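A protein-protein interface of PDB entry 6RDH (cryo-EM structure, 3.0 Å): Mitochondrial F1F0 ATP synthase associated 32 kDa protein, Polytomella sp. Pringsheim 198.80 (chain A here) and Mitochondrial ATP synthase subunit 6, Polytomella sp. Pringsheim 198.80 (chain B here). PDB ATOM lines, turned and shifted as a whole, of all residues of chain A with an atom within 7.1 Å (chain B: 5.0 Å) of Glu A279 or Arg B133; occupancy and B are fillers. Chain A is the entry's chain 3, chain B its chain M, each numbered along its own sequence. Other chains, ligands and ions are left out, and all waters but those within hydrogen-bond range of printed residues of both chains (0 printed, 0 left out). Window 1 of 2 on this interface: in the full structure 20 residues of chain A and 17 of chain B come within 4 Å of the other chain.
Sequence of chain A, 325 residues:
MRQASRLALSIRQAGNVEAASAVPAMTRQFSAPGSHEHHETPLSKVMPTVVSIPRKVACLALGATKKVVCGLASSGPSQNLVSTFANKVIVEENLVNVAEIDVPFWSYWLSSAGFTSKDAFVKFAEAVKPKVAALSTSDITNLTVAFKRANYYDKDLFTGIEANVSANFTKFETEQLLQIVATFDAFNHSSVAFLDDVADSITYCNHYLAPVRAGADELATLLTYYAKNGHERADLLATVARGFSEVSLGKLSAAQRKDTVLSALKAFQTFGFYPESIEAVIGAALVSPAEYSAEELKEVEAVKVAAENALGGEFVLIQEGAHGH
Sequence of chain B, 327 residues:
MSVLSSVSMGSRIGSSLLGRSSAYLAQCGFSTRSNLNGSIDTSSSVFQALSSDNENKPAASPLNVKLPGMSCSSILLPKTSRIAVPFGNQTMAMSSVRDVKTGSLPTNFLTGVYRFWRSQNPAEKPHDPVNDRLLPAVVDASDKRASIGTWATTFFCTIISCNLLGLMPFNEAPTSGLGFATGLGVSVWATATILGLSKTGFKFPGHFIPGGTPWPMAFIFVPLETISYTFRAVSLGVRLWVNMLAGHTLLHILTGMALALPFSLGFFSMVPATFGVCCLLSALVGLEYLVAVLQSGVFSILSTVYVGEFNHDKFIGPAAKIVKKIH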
ATOM      1  N   ALA A 241     -30.593 -26.115  19.722  1.00  0.00           N
ATOM      2  CA  ALA A 241     -30.301 -25.842  21.116  1.00  0.00           C
ATOM      3  C   ALA A 241     -31.395 -25.069  21.832  1.00  0.00           C
ATOM      4  O   ALA A 241     -31.357 -25.006  23.060  1.00  0.00           O
ATOM      5  CB  ALA A 241     -28.995 -25.074  21.218  1.00  0.00           C
ATOM      6  N   ARG A 242     -32.351 -24.469  21.119  1.00  0.00           N
ATOM      7  CA  ARG A 242     -33.528 -23.943  21.799  1.00  0.00           C
ATOM      8  C   ARG A 242     -34.363 -25.049  22.414  1.00  0.00           C
ATOM      9  O   ARG A 242     -34.960 -24.848  23.470  1.00  0.00           O
ATOM     10  CB  ARG A 242     -34.394 -23.118  20.856  1.00  0.00           C
ATOM     11  CG  ARG A 242     -34.013 -21.671  20.769  1.00  0.00           C
ATOM     12  CD  ARG A 242     -35.024 -20.919  19.949  1.00  0.00           C
ATOM     13  NE  ARG A 242     -34.898 -21.185  18.524  1.00  0.00           N
ATOM     14  CZ  ARG A 242     -34.149 -20.457  17.709  1.00  0.00           C
ATOM     15  NH1 ARG A 242     -34.079 -20.748  16.422  1.00  0.00           N
ATOM     16  NH2 ARG A 242     -33.468 -19.430  18.187  1.00  0.00           N
ATOM     17  N   PHE A 244     -33.585 -27.550  24.114  1.00  0.00           N
ATOM     18  CA  PHE A 244     -33.040 -28.112  25.344  1.00  0.00           C
ATOM     19  C   PHE A 244     -33.310 -27.135  26.475  1.00  0.00           C
ATOM     20  O   PHE A 244     -32.823 -26.003  26.457  1.00  0.00           O
ATOM     21  CB  PHE A 244     -31.545 -28.378  25.210  1.00  0.00           C
ATOM     22  CG  PHE A 244     -31.216 -29.487  24.271  1.00  0.00           C
ATOM     23  CD1 PHE A 244     -31.545 -30.787  24.581  1.00  0.00           C
ATOM     24  CD2 PHE A 244     -30.572 -29.231  23.084  1.00  0.00           C
ATOM     25  CE1 PHE A 244     -31.241 -31.807  23.717  1.00  0.00           C
ATOM     26  CE2 PHE A 244     -30.269 -30.250  22.219  1.00  0.00           C
ATOM     27  CZ  PHE A 244     -30.607 -31.535  22.535  1.00  0.00           C
ATOM     28  N   SER A 245     -34.082 -27.572  27.459  1.00  0.00           N
ATOM     29  CA  SER A 245     -34.395 -26.739  28.605  1.00  0.00           C
ATOM     30  C   SER A 245     -34.744 -27.639  29.777  1.00  0.00           C
ATOM     31  O   SER A 245     -34.688 -28.865  29.679  1.00  0.00           O
ATOM     32  CB  SER A 245     -35.543 -25.790  28.298  1.00  0.00           C
ATOM     33  OG  SER A 245     -36.744 -26.520  28.146  1.00  0.00           O
ATOM     34  N   GLU A 246     -35.108 -27.008  30.892  1.00  0.00           N
ATOM     35  CA  GLU A 246     -35.632 -27.747  32.032  1.00  0.00           C
ATOM     36  C   GLU A 246     -36.938 -28.435  31.688  1.00  0.00           C
ATOM     37  O   GLU A 246     -37.208 -29.536  32.178  1.00  0.00           O
ATOM     38  CB  GLU A 246     -35.846 -26.807  33.211  1.00  0.00           C
ATOM     39  CG  GLU A 246     -34.577 -26.363  33.883  1.00  0.00           C
ATOM     40  CD  GLU A 246     -33.949 -25.167  33.213  1.00  0.00           C
ATOM     41  OE1 GLU A 246     -34.609 -24.545  32.355  1.00  0.00           O
ATOM     42  OE2 GLU A 246     -32.787 -24.849  33.538  1.00  0.00           O
ATOM     43  N   VAL A 247     -37.741 -27.812  30.827  1.00  0.00           N
ATOM     44  CA  VAL A 247     -39.050 -28.344  30.479  1.00  0.00           C
ATOM     45  C   VAL A 247     -38.914 -29.587  29.617  1.00  0.00           C
ATOM     46  O   VAL A 247     -39.566 -30.605  29.863  1.00  0.00           O
ATOM     47  CB  VAL A 247     -39.879 -27.268  29.767  1.00  0.00           C
ATOM     48  CG1 VAL A 247     -41.296 -27.726  29.631  1.00  0.00           C
ATOM     49  CG2 VAL A 247     -39.790 -25.965  30.516  1.00  0.00           C
ATOM     50  N   LEU A 265     -24.205 -33.225  25.068  1.00  0.00           N
ATOM     51  CA  LEU A 265     -22.953 -32.584  25.461  1.00  0.00           C
ATOM     52  C   LEU A 265     -21.797 -33.038  24.584  1.00  0.00           C
ATOM     53  O   LEU A 265     -20.918 -32.234  24.251  1.00  0.00           O
ATOM     54  CB  LEU A 265     -22.646 -32.864  26.928  1.00  0.00           C
ATOM     55  CG  LEU A 265     -23.417 -32.043  27.953  1.00  0.00           C
ATOM     56  CD1 LEU A 265     -22.903 -32.344  29.323  1.00  0.00           C
ATOM     57  CD2 LEU A 265     -23.288 -30.572  27.669  1.00  0.00           C
ATOM     58  N   PRO A 275     -23.971 -22.707  23.187  1.00  0.00           N
ATOM     59  CA  PRO A 275     -25.026 -21.698  23.294  1.00  0.00           C
ATOM     60  C   PRO A 275     -25.381 -21.436  24.743  1.00  0.00           C
ATOM     61  O   PRO A 275     -24.906 -22.105  25.657  1.00  0.00           O
ATOM     62  CB  PRO A 275     -26.190 -22.350  22.561  1.00  0.00           C
ATOM     63  CG  PRO A 275     -25.981 -23.788  22.814  1.00  0.00           C
ATOM     64  CD  PRO A 275     -24.510 -24.013  22.783  1.00  0.00           C
ATOM     65  N   GLU A 276     -26.254 -20.447  24.945  1.00  0.00           N
ATOM     66  CA  GLU A 276     -26.686 -20.123  26.300  1.00  0.00           C
ATOM     67  C   GLU A 276     -27.535 -21.232  26.887  1.00  0.00           C
ATOM     68  O   GLU A 276     -27.534 -21.435  28.099  1.00  0.00           O
ATOM     69  CB  GLU A 276     -27.463 -18.812  26.319  1.00  0.00           C
ATOM     70  CG  GLU A 276     -27.577 -18.188  27.697  1.00  0.00           C
ATOM     71  CD  GLU A 276     -28.488 -16.980  27.721  1.00  0.00           C
ATOM     72  OE1 GLU A 276     -29.116 -16.687  26.683  1.00  0.00           O
ATOM     73  OE2 GLU A 276     -28.578 -16.321  28.776  1.00  0.00           O
ATOM     74  N   SER A 277     -28.221 -21.985  26.047  1.00  0.00           N
ATOM     75  CA  SER A 277     -29.072 -23.067  26.496  1.00  0.00           C
ATOM     76  C   SER A 277     -28.327 -24.377  26.673  1.00  0.00           C
ATOM     77  O   SER A 277     -28.968 -25.423  26.783  1.00  0.00           O
ATOM     78  CB  SER A 277     -30.219 -23.256  25.517  1.00  0.00           C
ATOM     79  OG  SER A 277     -30.804 -24.529  25.679  1.00  0.00           O
ATOM     80  N   ILE A 278     -26.991 -24.354  26.683  1.00  0.00           N
ATOM     81  CA  ILE A 278     -26.250 -25.547  27.083  1.00  0.00           C
ATOM     82  C   ILE A 278     -26.232 -25.683  28.593  1.00  0.00           C
ATOM     83  O   ILE A 278     -26.020 -26.785  29.108  1.00  0.00           O
ATOM     84  CB  ILE A 278     -24.821 -25.545  26.506  1.00  0.00           C
ATOM     85  CG1 ILE A 278     -24.322 -26.979  26.339  1.00  0.00           C
ATOM     86  CG2 ILE A 278     -23.851 -24.759  27.374  1.00  0.00           C
ATOM     87  CD1 ILE A 278     -22.960 -27.078  25.734  1.00  0.00           C
ATOM     88  N   GLU A 279     -26.502 -24.596  29.317  1.00  0.00           N
ATOM     89  CA  GLU A 279     -26.474 -24.642  30.764  1.00  0.00           C
ATOM     90  C   GLU A 279     -27.659 -25.410  31.314  1.00  0.00           C
ATOM     91  O   GLU A 279     -27.570 -25.948  32.414  1.00  0.00           O
ATOM     92  CB  GLU A 279     -26.415 -23.221  31.310  1.00  0.00           C
ATOM     93  CG  GLU A 279     -27.673 -22.434  31.148  1.00  0.00           C
ATOM     94  CD  GLU A 279     -27.443 -20.950  31.299  1.00  0.00           C
ATOM     95  OE1 GLU A 279     -26.271 -20.542  31.377  1.00  0.00           O
ATOM     96  OE2 GLU A 279     -28.429 -20.189  31.348  1.00  0.00           O
ATOM     97  N   ALA A 280     -28.728 -25.548  30.530  1.00  0.00           N
ATOM     98  CA  ALA A 280     -29.823 -26.429  30.905  1.00  0.00           C
ATOM     99  C   ALA A 280     -29.423 -27.892  30.772  1.00  0.00           C
ATOM    100  O   ALA A 280     -29.768 -28.713  31.628  1.00  0.00           O
ATOM    101  CB  ALA A 280     -31.040 -26.124  30.047  1.00  0.00           C
ATOM    102  N   VAL A 281     -28.671 -28.229  29.723  1.00  0.00           N
ATOM    103  CA  VAL A 281     -28.177 -29.593  29.552  1.00  0.00           C
ATOM    104  C   VAL A 281     -27.158 -29.932  30.633  1.00  0.00           C
ATOM    105  O   VAL A 281     -27.110 -31.062  31.129  1.00  0.00           O
ATOM    106  CB  VAL A 281     -27.580 -29.767  28.146  1.00  0.00           C
ATOM    107  CG1 VAL A 281     -27.326 -31.220  27.847  1.00  0.00           C
ATOM    108  CG2 VAL A 281     -28.500 -29.194  27.125  1.00  0.00           C
ATOM    109  N   ILE A 282     -26.341 -28.955  31.025  1.00  0.00           N
ATOM    110  CA  ILE A 282     -25.347 -29.192  32.066  1.00  0.00           C
ATOM    111  C   ILE A 282     -26.021 -29.323  33.425  1.00  0.00           C
ATOM    112  O   ILE A 282     -25.768 -30.277  34.171  1.00  0.00           O
ATOM    113  CB  ILE A 282     -24.288 -28.079  32.060  1.00  0.00           C
ATOM    114  CG1 ILE A 282     -23.491 -28.112  30.765  1.00  0.00           C
ATOM    115  CG2 ILE A 282     -23.331 -28.257  33.197  1.00  0.00           C
ATOM    116  CD1 ILE A 282     -22.604 -26.915  30.594  1.00  0.00           C
ATOM    117  N   GLY A 283     -26.918 -28.396  33.759  1.00  0.00           N
ATOM    118  CA  GLY A 283     -27.657 -28.461  35.004  1.00  0.00           C
ATOM    119  C   GLY A 283     -28.660 -29.589  35.090  1.00  0.00           C
ATOM    120  O   GLY A 283     -29.184 -29.835  36.177  1.00  0.00           O
ATOM    121  N   ALA A 284     -28.965 -30.258  33.978  1.00  0.00           N
ATOM    122  CA  ALA A 284     -29.710 -31.505  34.065  1.00  0.00           C
ATOM    123  C   ALA A 284     -28.869 -32.624  34.648  1.00  0.00           C
ATOM    124  O   ALA A 284     -29.424 -33.590  35.178  1.00  0.00           O
ATOM    125  CB  ALA A 284     -30.213 -31.919  32.688  1.00  0.00           C
ATOM    126  N   ALA A 285     -27.549 -32.517  34.546  1.00  0.00           N
ATOM    127  CA  ALA A 285     -26.629 -33.470  35.143  1.00  0.00           C
ATOM    128  C   ALA A 285     -26.119 -33.027  36.501  1.00  0.00           C
ATOM    129  O   ALA A 285     -25.914 -33.867  37.378  1.00  0.00           O
ATOM    130  CB  ALA A 285     -25.438 -33.699  34.211  1.00  0.00           C
ATOM    131  N   ALA A 307     -17.735 -24.334  28.263  1.00  0.00           N
ATOM    132  CA  ALA A 307     -18.858 -23.419  28.161  1.00  0.00           C
ATOM    133  C   ALA A 307     -18.774 -22.274  29.155  1.00  0.00           C
ATOM    134  O   ALA A 307     -19.374 -21.226  28.913  1.00  0.00           O
ATOM    135  CB  ALA A 307     -20.165 -24.180  28.363  1.00  0.00           C
ATOM    136  N   LEU A 311     -19.012 -18.874  27.121  1.00  0.00           N
ATOM    137  CA  LEU A 311     -20.074 -17.940  27.468  1.00  0.00           C
ATOM    138  C   LEU A 311     -19.609 -16.818  28.383  1.00  0.00           C
ATOM    139  O   LEU A 311     -20.416 -15.950  28.725  1.00  0.00           O
ATOM    140  CB  LEU A 311     -21.243 -18.686  28.112  1.00  0.00           C
ATOM    141  CG  LEU A 311     -22.114 -19.442  27.108  1.00  0.00           C
ATOM    142  CD1 LEU A 311     -22.647 -20.723  27.691  1.00  0.00           C
ATOM    143  CD2 LEU A 311     -23.253 -18.560  26.656  1.00  0.00           C
ATOM    144  N   PHE A 315     -20.332 -20.985  36.087  1.00  0.00           N
ATOM    145  CA  PHE A 315     -21.540 -21.775  36.268  1.00  0.00           C
ATOM    146  C   PHE A 315     -22.039 -21.686  37.702  1.00  0.00           C
ATOM    147  O   PHE A 315     -21.251 -21.616  38.648  1.00  0.00           O
ATOM    148  CB  PHE A 315     -21.267 -23.228  35.907  1.00  0.00           C
ATOM    149  CG  PHE A 315     -22.488 -23.992  35.529  1.00  0.00           C
ATOM    150  CD1 PHE A 315     -22.875 -24.077  34.207  1.00  0.00           C
ATOM    151  CD2 PHE A 315     -23.241 -24.637  36.486  1.00  0.00           C
ATOM    152  CE1 PHE A 315     -23.998 -24.778  33.848  1.00  0.00           C
ATOM    153  CE2 PHE A 315     -24.366 -25.340  36.131  1.00  0.00           C
ATOM    154  CZ  PHE A 315     -24.744 -25.411  34.812  1.00  0.00           C
ATOM    155  N   VAL A 316     -23.358 -21.697  37.858  1.00  0.00           N
ATOM    156  CA  VAL A 316     -23.990 -21.645  39.172  1.00  0.00           C
ATOM    157  C   VAL A 316     -25.341 -22.344  39.096  1.00  0.00           C
ATOM    158  O   VAL A 316     -26.154 -22.053  38.216  1.00  0.00           O
ATOM    159  CB  VAL A 316     -24.110 -20.187  39.674  1.00  0.00           C
ATOM    160  CG1 VAL A 316     -24.594 -19.256  38.577  1.00  0.00           C
ATOM    161  CG2 VAL A 316     -25.034 -20.103  40.867  1.00  0.00           C
ATOM    162  N   ASN B 131     -35.180 -14.503  26.261  1.00  0.00           N
ATOM    163  CA  ASN B 131     -34.278 -14.768  25.150  1.00  0.00           C
ATOM    164  C   ASN B 131     -34.422 -16.244  24.811  1.00  0.00           C
ATOM    165  O   ASN B 131     -35.411 -16.878  25.188  1.00  0.00           O
ATOM    166  CB  ASN B 131     -32.850 -14.318  25.489  1.00  0.00           C
ATOM    167  CG  ASN B 131     -32.331 -14.899  26.788  1.00  0.00           C
ATOM    168  OD1 ASN B 131     -32.977 -15.717  27.437  1.00  0.00           O
ATOM    169  ND2 ASN B 131     -31.146 -14.460  27.181  1.00  0.00           N
ATOM    170  N   ASP B 132     -33.455 -16.802  24.076  1.00  0.00           N
ATOM    171  CA  ASP B 132     -33.509 -18.217  23.715  1.00  0.00           C
ATOM    172  C   ASP B 132     -33.413 -19.143  24.918  1.00  0.00           C
ATOM    173  O   ASP B 132     -33.849 -20.293  24.832  1.00  0.00           O
ATOM    174  CB  ASP B 132     -32.387 -18.572  22.748  1.00  0.00           C
ATOM    175  CG  ASP B 132     -32.486 -17.837  21.437  1.00  0.00           C
ATOM    176  OD1 ASP B 132     -32.197 -16.623  21.413  1.00  0.00           O
ATOM    177  OD2 ASP B 132     -32.836 -18.477  20.425  1.00  0.00           O
ATOM    178  N   ARG B 133     -32.841 -18.677  26.025  1.00  0.00           N
ATOM    179  CA  ARG B 133     -32.799 -19.483  27.237  1.00  0.00           C
ATOM    180  C   ARG B 133     -34.183 -19.622  27.854  1.00  0.00           C
ATOM    181  O   ARG B 133     -34.566 -20.710  28.295  1.00  0.00           O
ATOM    182  CB  ARG B 133     -31.824 -18.859  28.231  1.00  0.00           C
ATOM    183  CG  ARG B 133     -31.682 -19.610  29.541  1.00  0.00           C
ATOM    184  CD  ARG B 133     -31.005 -20.944  29.349  1.00  0.00           C
ATOM    185  NE  ARG B 133     -30.920 -21.683  30.598  1.00  0.00           N
ATOM    186  CZ  ARG B 133     -31.722 -22.690  30.917  1.00  0.00           C
ATOM    187  NH1 ARG B 133     -32.663 -23.073  30.073  1.00  0.00           N
ATOM    188  NH2 ARG B 133     -31.580 -23.316  32.072  1.00  0.00           N
ATOM    189  N   LEU B 134     -34.953 -18.540  27.875  1.00  0.00           N
ATOM    190  CA  LEU B 134     -36.251 -18.526  28.529  1.00  0.00           C
ATOM    191  C   LEU B 134     -37.400 -18.907  27.609  1.00  0.00           C
ATOM    192  O   LEU B 134     -38.521 -19.074  28.093  1.00  0.00           O
ATOM    193  CB  LEU B 134     -36.518 -17.143  29.115  1.00  0.00           C
ATOM    194  CG  LEU B 134     -37.319 -17.117  30.411  1.00  0.00           C
ATOM    195  CD1 LEU B 134     -36.603 -17.893  31.482  1.00  0.00           C
ATOM    196  CD2 LEU B 134     -37.549 -15.702  30.842  1.00  0.00           C
ATOM    197  N   LEU B 135     -37.159 -19.058  26.315  1.00  0.00           N
ATOM    198  CA  LEU B 135     -38.207 -19.353  25.343  1.00  0.00           C
ATOM    199  C   LEU B 135     -38.947 -20.674  25.548  1.00  0.00           C
ATOM    200  O   LEU B 135     -40.163 -20.687  25.337  1.00  0.00           O
ATOM    201  CB  LEU B 135     -37.650 -19.314  23.923  1.00  0.00           C
ATOM    202  CG  LEU B 135     -37.800 -18.010  23.160  1.00  0.00           C
ATOM    203  CD1 LEU B 135     -37.300 -18.218  21.762  1.00  0.00           C
ATOM    204  CD2 LEU B 135     -39.229 -17.533  23.169  1.00  0.00           C
ATOM    205  N   PRO B 136     -38.319 -21.798  25.930  1.00  0.00           N
ATOM    206  CA  PRO B 136     -39.153 -22.963  26.247  1.00  0.00           C
ATOM    207  C   PRO B 136     -39.940 -22.804  27.520  1.00  0.00           C
ATOM    208  O   PRO B 136     -41.025 -23.377  27.623  1.00  0.00           O
ATOM    209  CB  PRO B 136     -38.146 -24.109  26.354  1.00  0.00           C
ATOM    210  CG  PRO B 136     -37.004 -23.661  25.633  1.00  0.00           C
ATOM    211  CD  PRO B 136     -36.906 -22.217  25.876  1.00  0.00           C
ATOM    212  N   PRO B 318     -35.091 -21.133  34.490  1.00  0.00           N
ATOM    213  CA  PRO B 318     -33.792 -21.808  34.447  1.00  0.00           C
ATOM    214  C   PRO B 318     -33.328 -22.300  35.808  1.00  0.00           C
ATOM    215  O   PRO B 318     -33.279 -21.543  36.781  1.00  0.00           O
ATOM    216  CB  PRO B 318     -32.862 -20.732  33.884  1.00  0.00           C
ATOM    217  CG  PRO B 318     -33.478 -19.475  34.259  1.00  0.00           C
ATOM    218  CD  PRO B 318     -34.954 -19.676  34.355  1.00  0.00           C
ATOM    219  N   ALA B 319     -32.986 -23.581  35.879  1.00  0.00           N
ATOM    220  CA  ALA B 319     -32.459 -24.191  37.086  1.00  0.00           C
ATOM    221  C   ALA B 319     -30.937 -24.205  37.123  1.00  0.00           C
ATOM    222  O   ALA B 319     -30.356 -24.841  38.005  1.00  0.00           O
ATOM    223  CB  ALA B 319     -33.000 -25.614  37.229  1.00  0.00           C
ATOM    224  N   ALA B 320     -30.289 -23.522  36.188  1.00  0.00           N
ATOM    225  CA  ALA B 320     -28.841 -23.427  36.122  1.00  0.00           C
ATOM    226  C   ALA B 320     -28.500 -22.206  35.294  1.00  0.00           C
ATOM    227  O   ALA B 320     -29.269 -21.807  34.420  1.00  0.00           O
ATOM    228  CB  ALA B 320     -28.218 -24.680  35.506  1.00  0.00           C
ATOM    229  N   LYS B 321     -27.346 -21.614  35.568  1.00  0.00           N
ATOM    230  CA  LYS B 321     -27.017 -20.361  34.914  1.00  0.00           C
ATOM    231  C   LYS B 321     -25.508 -20.218  34.822  1.00  0.00           C
ATOM    232  O   LYS B 321     -24.766 -20.822  35.597  1.00  0.00           O
ATOM    233  CB  LYS B 321     -27.629 -19.178  35.671  1.00  0.00           C
ATOM    234  CG  LYS B 321     -27.882 -17.956  34.817  1.00  0.00           C
ATOM    235  CD  LYS B 321     -28.456 -16.811  35.624  1.00  0.00           C
ATOM    236  CE  LYS B 321     -28.338 -15.512  34.852  1.00  0.00           C
ATOM    237  NZ  LYS B 321     -28.841 -15.653  33.456  1.00  0.00           N
ATOM    238  N   ILE B 322     -25.063 -19.441  33.842  1.00  0.00           N
ATOM    239  CA  ILE B 322     -23.669 -19.033  33.728  1.00  0.00           C
ATOM    240  C   ILE B 322     -23.625 -17.521  33.899  1.00  0.00           C
ATOM    241  O   ILE B 322     -23.864 -16.765  32.953  1.00  0.00           O
ATOM    242  CB  ILE B 322     -23.066 -19.500  32.394  1.00  0.00           C
ATOM    243  CG1 ILE B 322     -23.117 -21.027  32.327  1.00  0.00           C
ATOM    244  CG2 ILE B 322     -21.654 -19.000  32.231  1.00  0.00           C
ATOM    245  CD1 ILE B 322     -22.259 -21.660  31.268  1.00  0.00           C
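Among the printed residues, merely in contact across the chains: Arg A242 with Pro B136 (3.2 Å), Ser A245 with Pro B136 (3.3 Å), Glu A246 with Pro B318 (3.3 Å), Glu A279 with Ala B320 (3.4 Å), Phe A315 with Lys B321 (3.4 Å), Ala A280 with Arg B133 (3.5 Å), Glu A279 with Lys B321 (3.5 Å), Phe A315 with Ile B322 (3.6 Å), Phe A315 with Ala B320 (3.6 Å), Val A316 with Ala B320 (3.7 Å), Leu A311 with Ile B322 (3.7 Å), Glu A276 with Arg B133 (3.7 Å), Ala A307 with Ile B322 (3.7 Å), Gly A283 with Ala B320 (3.9 Å), Glu A246 with Ala B320 (3.9 Å) and Arg A242 with Leu B135 (3.97 Å).
OE1 of Glu A276 is in hydrogen-bond range of ND2 of Asn B131, 3.1 Å away. OD2 of Asp B132 is in salt-bridge range of NH2 of Arg A242. NH2 of Arg B133 is in salt-bridge range of OE2 of Glu A246, at 2.4 Å. N of Val A316 lies within hydrogen-bond range of O of Lys B321 (2.8 Å). OE2 of Glu A279 lies within salt-bridge range of NE of Arg B133, 3.0 Å away. The backbone NH of Ala B319 lies within hydrogen-bond range of the side-chain carboxylate of Glu A246. The side-chain carboxylate (OE1) of Glu A279 is in hydrogen-bond range of the backbone NH (N) of Ile B322, at 3.0 Å.
N of Val A247 lies within hydrogen-bond range of OG of Ser A245 (3.1 Å). The backbone NH (N) of Leu B134 sits at hydrogen-bond distance from the side-chain amide oxygen (OD1) of Asn B131, 3.5 Å away. OD1 of Asn B131 lies close to N of Arg B133 (3.3 Å).
Of the 11 printed residues of chain B, 10 touch a printed residue of chain A. Printed residues of chain B that touch a printed residue of chain A: Asn B131, Asp B132, Arg B133, Leu B135, Pro B136, Pro B318, Ala B319, Ala B320, Lys B321 and Ile B322. Hydrophobic or aromatic side chains of chain B that line the printed part of chain A: Leu B135, Pro B136, Ala B319, Ala B320 and Ile B322. Of the 22 printed residues of chain A, 11 touch a printed residue of chain B. Hydrophobic or aromatic side chains of chain A within 4 Å of the printed part of chain B: Ala A280, Leu A311, Phe A315 and Val A316. Among the printed residues, Asp or Glu carboxylates within 4 Å of a Lys or Arg side-chain nitrogen of the other chain: Arg A242 with Asp B132 (2.5 Å), Glu A246 with Arg B133 (2.4 Å) and Glu A279 with Arg B133 (3.0 Å).
Of chain B, only Arg B133, Ala B320, Lys B321 and Ile B322 come within 4 Å of Glu A279. Printed residues of chain A within 4 Å of Ala B319: Glu A246 (2.7 Å). Of the printed residues of chain B, Arg A242 touches Asp B132, Leu B135 and Pro B136. Of the printed residues of chain B, Ser A245 touches Pro B136 (3.3 Å). Ile A282 touches none of the printed residues of chain B. Val A247 touches none of the printed residues of chain B. The nearest printed residue of chain B that does not touch Glu A279 is Pro B318 (5.1 Å). The nearest residue of chain A that does not touch Arg B133 is Ser A277 (4.05 Å).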
